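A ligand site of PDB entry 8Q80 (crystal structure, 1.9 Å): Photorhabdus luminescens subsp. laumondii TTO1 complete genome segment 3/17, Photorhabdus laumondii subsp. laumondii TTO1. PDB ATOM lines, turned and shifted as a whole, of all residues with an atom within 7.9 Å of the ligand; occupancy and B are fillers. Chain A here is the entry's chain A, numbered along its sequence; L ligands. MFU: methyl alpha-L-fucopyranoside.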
ATOM      1  N   ASN A 150     -21.736  -6.605  -1.069  1.00  0.00           N
ATOM      2  CA  ASN A 150     -22.293  -7.828  -0.490  1.00  0.00           C
ATOM      3  C   ASN A 150     -23.303  -7.537   0.619  1.00  0.00           C
ATOM      4  O   ASN A 150     -23.723  -8.461   1.316  1.00  0.00           O
ATOM      5  CB  ASN A 150     -21.235  -8.798   0.030  1.00  0.00           C
ATOM      6  CG  ASN A 150     -20.449  -9.464  -1.076  1.00  0.00           C
ATOM      7  OD1 ASN A 150     -21.019  -9.954  -2.046  1.00  0.00           O
ATOM      8  ND2 ASN A 150     -19.132  -9.456  -0.956  1.00  0.00           N
ATOM      9  N   ALA A 151     -23.711  -6.263   0.779  1.00  0.00           N
ATOM     10  CA  ALA A 151     -24.891  -5.923   1.548  1.00  0.00           C
ATOM     11  C   ALA A 151     -26.152  -6.267   0.751  1.00  0.00           C
ATOM     12  O   ALA A 151     -26.118  -6.395  -0.474  1.00  0.00           O
ATOM     13  CB  ALA A 151     -24.908  -4.454   1.876  1.00  0.00           C
ATOM     14  N   LEU A 171     -29.694  -2.152   3.032  1.00  0.00           N
ATOM     15  CA  LEU A 171     -30.262  -2.650   4.267  1.00  0.00           C
ATOM     16  C   LEU A 171     -29.126  -3.321   5.021  1.00  0.00           C
ATOM     17  O   LEU A 171     -29.364  -4.088   5.946  1.00  0.00           O
ATOM     18  CB  LEU A 171     -31.437  -3.608   3.981  1.00  0.00           C
ATOM     19  CG  LEU A 171     -32.609  -2.997   3.215  1.00  0.00           C
ATOM     20  CD1 LEU A 171     -33.655  -4.049   2.875  1.00  0.00           C
ATOM     21  CD2 LEU A 171     -33.233  -1.834   3.981  1.00  0.00           C
ATOM     22  N   ASN A 172     -27.902  -3.030   4.586  1.00  0.00           N
ATOM     23  CA  ASN A 172     -26.713  -3.402   5.308  1.00  0.00           C
ATOM     24  C   ASN A 172     -26.578  -4.928   5.295  1.00  0.00           C
ATOM     25  O   ASN A 172     -27.089  -5.592   4.378  1.00  0.00           O
ATOM     26  CB  ASN A 172     -26.724  -2.710   6.676  1.00  0.00           C
ATOM     27  CG  ASN A 172     -26.867  -1.213   6.510  1.00  0.00           C
ATOM     28  OD1 ASN A 172     -25.925  -0.558   6.069  1.00  0.00           O
ATOM     29  ND2 ASN A 172     -28.035  -0.670   6.826  1.00  0.00           N
ATOM     30  N   GLY A 173     -25.844  -5.444   6.291  1.00  0.00           N
ATOM     31  CA  GLY A 173     -25.464  -6.847   6.372  1.00  0.00           C
ATOM     32  C   GLY A 173     -24.405  -7.223   5.349  1.00  0.00           C
ATOM     33  O   GLY A 173     -24.046  -6.418   4.489  1.00  0.00           O
ATOM     34  N   VAL A 174     -23.881  -8.446   5.516  1.00  0.00           N
ATOM     35  CA  VAL A 174     -22.995  -9.097   4.567  1.00  0.00           C
ATOM     36  C   VAL A 174     -23.524 -10.506   4.332  1.00  0.00           C
ATOM     37  O   VAL A 174     -23.611 -11.296   5.275  1.00  0.00           O
ATOM     38  CB  VAL A 174     -21.516  -9.125   5.031  1.00  0.00           C
ATOM     39  CG1 VAL A 174     -20.605  -9.740   3.969  1.00  0.00           C
ATOM     40  CG2 VAL A 174     -21.010  -7.735   5.411  1.00  0.00           C
ATOM     41  N   ILE A 175     -23.921 -10.807   3.085  1.00  0.00           N
ATOM     42  CA  ILE A 175     -24.668 -12.029   2.811  1.00  0.00           C
ATOM     43  C   ILE A 175     -23.990 -12.812   1.708  1.00  0.00           C
ATOM     44  O   ILE A 175     -23.307 -12.238   0.875  1.00  0.00           O
ATOM     45  CB  ILE A 175     -26.161 -11.728   2.495  1.00  0.00           C
ATOM     46  CG1 ILE A 175     -26.327 -10.875   1.218  1.00  0.00           C
ATOM     47  CG2 ILE A 175     -26.826 -11.084   3.704  1.00  0.00           C
ATOM     48  CD1 ILE A 175     -27.754 -10.745   0.726  1.00  0.00           C
ATOM     49  N   THR A 176     -24.182 -14.136   1.736  1.00  0.00           N
ATOM     50  CA  THR A 176     -23.449 -15.087   0.916  1.00  0.00           C
ATOM     51  C   THR A 176     -24.389 -16.049   0.187  1.00  0.00           C
ATOM     52  O   THR A 176     -23.914 -17.045  -0.340  1.00  0.00           O
ATOM     53  CB  THR A 176     -22.497 -15.902   1.794  1.00  0.00           C
ATOM     54  OG1 THR A 176     -23.242 -16.672   2.747  1.00  0.00           O
ATOM     55  CG2 THR A 176     -21.504 -15.006   2.521  1.00  0.00           C
ATOM     56  N   ALA A 193     -31.389 -14.514   4.319  1.00  0.00           N
ATOM     57  CA  ALA A 193     -30.205 -14.763   3.511  1.00  0.00           C
ATOM     58  C   ALA A 193     -29.141 -15.409   4.406  1.00  0.00           C
ATOM     59  O   ALA A 193     -29.163 -15.242   5.623  1.00  0.00           O
ATOM     60  CB  ALA A 193     -29.705 -13.477   2.888  1.00  0.00           C
ATOM     61  N   ARG A 194     -28.263 -16.197   3.796  1.00  0.00           N
ATOM     62  CA  ARG A 194     -27.124 -16.767   4.521  1.00  0.00           C
ATOM     63  C   ARG A 194     -26.056 -15.714   4.772  1.00  0.00           C
ATOM     64  O   ARG A 194     -25.825 -14.835   3.945  1.00  0.00           O
ATOM     65  CB  ARG A 194     -26.484 -17.889   3.716  1.00  0.00           C
ATOM     66  CG  ARG A 194     -25.448 -18.704   4.479  1.00  0.00           C
ATOM     67  CD  ARG A 194     -25.035 -19.886   3.627  1.00  0.00           C
ATOM     68  NE  ARG A 194     -24.291 -19.420   2.476  1.00  0.00           N
ATOM     69  CZ  ARG A 194     -23.792 -20.225   1.557  1.00  0.00           C
ATOM     70  NH1 ARG A 194     -23.932 -21.537   1.664  1.00  0.00           N
ATOM     71  NH2 ARG A 194     -23.153 -19.718   0.531  1.00  0.00           N
ATOM     72  N   GLY A 195     -25.428 -15.799   5.937  1.00  0.00           N
ATOM     73  CA  GLY A 195     -24.423 -14.837   6.343  1.00  0.00           C
ATOM     74  C   GLY A 195     -23.016 -15.398   6.141  1.00  0.00           C
ATOM     75  O   GLY A 195     -22.842 -16.533   5.660  1.00  0.00           O
ATOM     76  N   THR A 196     -22.016 -14.585   6.533  1.00  0.00           N
ATOM     77  CA  THR A 196     -20.624 -14.907   6.305  1.00  0.00           C
ATOM     78  C   THR A 196     -20.203 -16.055   7.204  1.00  0.00           C
ATOM     79  O   THR A 196     -19.193 -16.699   6.933  1.00  0.00           O
ATOM     80  CB  THR A 196     -19.724 -13.671   6.461  1.00  0.00           C
ATOM     81  OG1 THR A 196     -19.874 -13.211   7.805  1.00  0.00           O
ATOM     82  CG2 THR A 196     -20.099 -12.559   5.509  1.00  0.00           C
ATOM     83  N   ASP A 197     -21.015 -16.386   8.212  1.00  0.00           N
ATOM     84  CA  ASP A 197     -20.748 -17.529   9.083  1.00  0.00           C
ATOM     85  C   ASP A 197     -21.546 -18.752   8.641  1.00  0.00           C
ATOM     86  O   ASP A 197     -21.577 -19.749   9.371  1.00  0.00           O
ATOM     87  CB  ASP A 197     -21.075 -17.182  10.541  1.00  0.00           C
ATOM     88  CG  ASP A 197     -22.486 -16.620  10.752  1.00  0.00           C
ATOM     89  OD1 ASP A 197     -23.259 -16.513   9.749  1.00  0.00           O
ATOM     90  OD2 ASP A 197     -22.816 -16.268  11.910  1.00  0.00           O
ATOM     91  N   ASN A 198     -22.231 -18.666   7.493  1.00  0.00           N
ATOM     92  CA  ASN A 198     -23.053 -19.734   6.938  1.00  0.00           C
ATOM     93  C   ASN A 198     -24.345 -19.973   7.724  1.00  0.00           C
ATOM     94  O   ASN A 198     -25.063 -20.947   7.466  1.00  0.00           O
ATOM     95  CB  ASN A 198     -22.286 -21.029   6.750  1.00  0.00           C
ATOM     96  CG  ASN A 198     -21.369 -20.961   5.546  1.00  0.00           C
ATOM     97  OD1 ASN A 198     -21.727 -20.417   4.515  1.00  0.00           O
ATOM     98  ND2 ASN A 198     -20.179 -21.502   5.672  1.00  0.00           N
ATOM     99  N   ALA A 199     -24.686 -19.050   8.642  1.00  0.00           N
ATOM    100  CA  ALA A 199     -25.918 -19.147   9.400  1.00  0.00           C
ATOM    101  C   ALA A 199     -27.032 -18.496   8.559  1.00  0.00           C
ATOM    102  O   ALA A 199     -26.737 -17.723   7.649  1.00  0.00           O
ATOM    103  CB  ALA A 199     -25.765 -18.480  10.758  1.00  0.00           C
ATOM    104  N   LEU A 200     -28.289 -18.884   8.819  1.00  0.00           N
ATOM    105  CA  LEU A 200     -29.459 -18.144   8.343  1.00  0.00           C
ATOM    106  C   LEU A 200     -29.632 -16.864   9.156  1.00  0.00           C
ATOM    107  O   LEU A 200     -29.781 -16.936  10.365  1.00  0.00           O
ATOM    108  CB  LEU A 200     -30.679 -19.053   8.531  1.00  0.00           C
ATOM    109  CG  LEU A 200     -32.008 -18.405   8.109  1.00  0.00           C
ATOM    110  CD1 LEU A 200     -32.011 -18.144   6.613  1.00  0.00           C
ATOM    111  CD2 LEU A 200     -33.200 -19.248   8.548  1.00  0.00           C
ATOM    112  N   TRP A 201     -29.595 -15.703   8.503  1.00  0.00           N
ATOM    113  CA  TRP A 201     -29.953 -14.439   9.108  1.00  0.00           C
ATOM    114  C   TRP A 201     -31.232 -13.865   8.494  1.00  0.00           C
ATOM    115  O   TRP A 201     -31.659 -14.272   7.419  1.00  0.00           O
ATOM    116  CB  TRP A 201     -28.803 -13.454   8.915  1.00  0.00           C
ATOM    117  CG  TRP A 201     -27.518 -13.849   9.573  1.00  0.00           C
ATOM    118  CD1 TRP A 201     -26.711 -14.910   9.295  1.00  0.00           C
ATOM    119  CD2 TRP A 201     -26.887 -13.147  10.654  1.00  0.00           C
ATOM    120  NE1 TRP A 201     -25.626 -14.910  10.126  1.00  0.00           N
ATOM    121  CE2 TRP A 201     -25.699 -13.830  10.957  1.00  0.00           C
ATOM    122  CE3 TRP A 201     -27.212 -11.998  11.372  1.00  0.00           C
ATOM    123  CZ2 TRP A 201     -24.819 -13.401  11.956  1.00  0.00           C
ATOM    124  CZ3 TRP A 201     -26.348 -11.574  12.375  1.00  0.00           C
ATOM    125  CH2 TRP A 201     -25.167 -12.259  12.642  1.00  0.00           C
ATOM    126  N   HIS A 202     -31.804 -12.844   9.163  1.00  0.00           N
ATOM    127  CA  HIS A 202     -33.025 -12.213   8.682  1.00  0.00           C
ATOM    128  C   HIS A 202     -33.118 -10.788   9.188  1.00  0.00           C
ATOM    129  O   HIS A 202     -32.502 -10.443  10.192  1.00  0.00           O
ATOM    130  CB  HIS A 202     -34.277 -13.049   9.003  1.00  0.00           C
ATOM    131  CG  HIS A 202     -34.630 -13.193  10.445  1.00  0.00           C
ATOM    132  ND1 HIS A 202     -35.928 -13.195  10.921  1.00  0.00           N
ATOM    133  CD2 HIS A 202     -33.852 -13.395  11.491  1.00  0.00           C
ATOM    134  CE1 HIS A 202     -35.906 -13.342  12.228  1.00  0.00           C
ATOM    135  NE2 HIS A 202     -34.652 -13.480  12.595  1.00  0.00           N
ATOM    136  N   GLY A 215     -32.482  -4.648  12.580  1.00  0.00           N
ATOM    137  CA  GLY A 215     -31.137  -5.154  12.411  1.00  0.00           C
ATOM    138  C   GLY A 215     -31.209  -6.600  11.940  1.00  0.00           C
ATOM    139  O   GLY A 215     -32.228  -7.247  12.134  1.00  0.00           O
ATOM    140  N   TRP A 216     -30.127  -7.058  11.322  1.00  0.00           N
ATOM    141  CA  TRP A 216     -29.932  -8.465  11.018  1.00  0.00           C
ATOM    142  C   TRP A 216     -29.856  -9.291  12.305  1.00  0.00           C
ATOM    143  O   TRP A 216     -28.982  -9.092  13.142  1.00  0.00           O
ATOM    144  CB  TRP A 216     -28.694  -8.652  10.141  1.00  0.00           C
ATOM    145  CG  TRP A 216     -28.890  -8.197   8.727  1.00  0.00           C
ATOM    146  CD1 TRP A 216     -28.616  -6.959   8.213  1.00  0.00           C
ATOM    147  CD2 TRP A 216     -29.384  -8.989   7.628  1.00  0.00           C
ATOM    148  NE1 TRP A 216     -28.966  -6.907   6.881  1.00  0.00           N
ATOM    149  CE2 TRP A 216     -29.413  -8.158   6.495  1.00  0.00           C
ATOM    150  CE3 TRP A 216     -29.842 -10.311   7.509  1.00  0.00           C
ATOM    151  CZ2 TRP A 216     -29.840  -8.620   5.246  1.00  0.00           C
ATOM    152  CZ3 TRP A 216     -30.303 -10.763   6.288  1.00  0.00           C
ATOM    153  CH2 TRP A 216     -30.304  -9.925   5.178  1.00  0.00           C
ATOM    154  N   ASP A 217     -30.730 -10.295  12.396  1.00  0.00           N
ATOM    155  CA  ASP A 217     -30.805 -11.229  13.489  1.00  0.00           C
ATOM    156  C   ASP A 217     -30.338 -12.572  12.953  1.00  0.00           C
ATOM    157  O   ASP A 217     -30.740 -12.942  11.841  1.00  0.00           O
ATOM    158  CB  ASP A 217     -32.249 -11.369  13.996  1.00  0.00           C
ATOM    159  CG  ASP A 217     -32.434 -12.359  15.131  1.00  0.00           C
ATOM    160  OD1 ASP A 217     -31.792 -12.115  16.154  1.00  0.00           O
ATOM    161  OD2 ASP A 217     -33.226 -13.391  14.986  1.00  0.00           O
ATOM    162  N   SER A 218     -29.532 -13.302  13.744  1.00  0.00           N
ATOM    163  CA  SER A 218     -29.104 -14.636  13.366  1.00  0.00           C
ATOM    164  C   SER A 218     -30.100 -15.659  13.868  1.00  0.00           C
ATOM    165  O   SER A 218     -30.408 -15.679  15.032  1.00  0.00           O
ATOM    166  CB  SER A 218     -27.728 -14.985  13.864  1.00  0.00           C
ATOM    167  OG  SER A 218     -27.368 -16.291  13.407  1.00  0.00           O
HETATM  168  C1  MFU L   1     -23.261  -8.962   8.973  1.00  0.00           C
HETATM  169  C2  MFU L   1     -22.035  -9.863   9.134  1.00  0.00           C
HETATM  170  C3  MFU L   1     -22.413 -11.235   9.676  1.00  0.00           C
HETATM  171  C4  MFU L   1     -23.535 -11.854   8.845  1.00  0.00           C
HETATM  172  C5  MFU L   1     -24.714 -10.881   8.734  1.00  0.00           C
HETATM  173  C6  MFU L   1     -25.799 -11.373   7.810  1.00  0.00           C
HETATM  174  O1  MFU L   1     -23.743  -8.624  10.248  1.00  0.00           O
HETATM  175  O2  MFU L   1     -21.089  -9.216  10.002  1.00  0.00           O
HETATM  176  O3  MFU L   1     -21.291 -12.115   9.676  1.00  0.00           O
HETATM  177  O4  MFU L   1     -22.983 -12.210   7.560  1.00  0.00           O
HETATM  178  O5  MFU L   1     -24.256  -9.620   8.193  1.00  0.00           O
HETATM  179  CM  MFU L   1     -24.917  -7.796  10.228  1.00  0.00           C
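Merely in contact with the ligand: Gly 195, Trp 201, Gly 173 and Trp 216.
Within 4 Å of the ligand: Gly 173, Val 174, Gly 195, Thr 196, Trp 201 and Trp 216.
The nearest printed residue that does not touch the ligand is Ile 175 (4.2 Å).
An oxygen (O5) of the ligand sits at hydrogen-bond distance from the backbone NH (N) of Val 174, at 2.9 Å.
O of Val 174 sits at hydrogen-bond distance from O4 of the ligand.
O4 of the ligand sits at hydrogen-bond distance from N of Thr 196 (2.8 Å).
The side-chain hydroxyl (OG1) of Thr 196 is in hydrogen-bond range of an oxygen (O3) of the ligand.
The side-chain hydroxyl (OG1) of Thr 176 sits at hydrogen-bond distance from the backbone carbonyl oxygen (O) of Gly 195, 2.9 Å away.
The indole nitrogen of Trp 201 sits at hydrogen-bond distance from the side-chain carboxylate of Asp 197.
N of Trp 201 sits at hydrogen-bond distance from O of Ala 193 (2.9 Å).
The indole nitrogen (NE1) of Trp 216 is in hydrogen-bond range of the backbone carbonyl oxygen (O) of Asn 172, at 3.4 Å.
The backbone carbonyl oxygen (O) of Leu 171 is in hydrogen-bond range of the indole nitrogen (NE1) of Trp 216 (3.0 Å).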
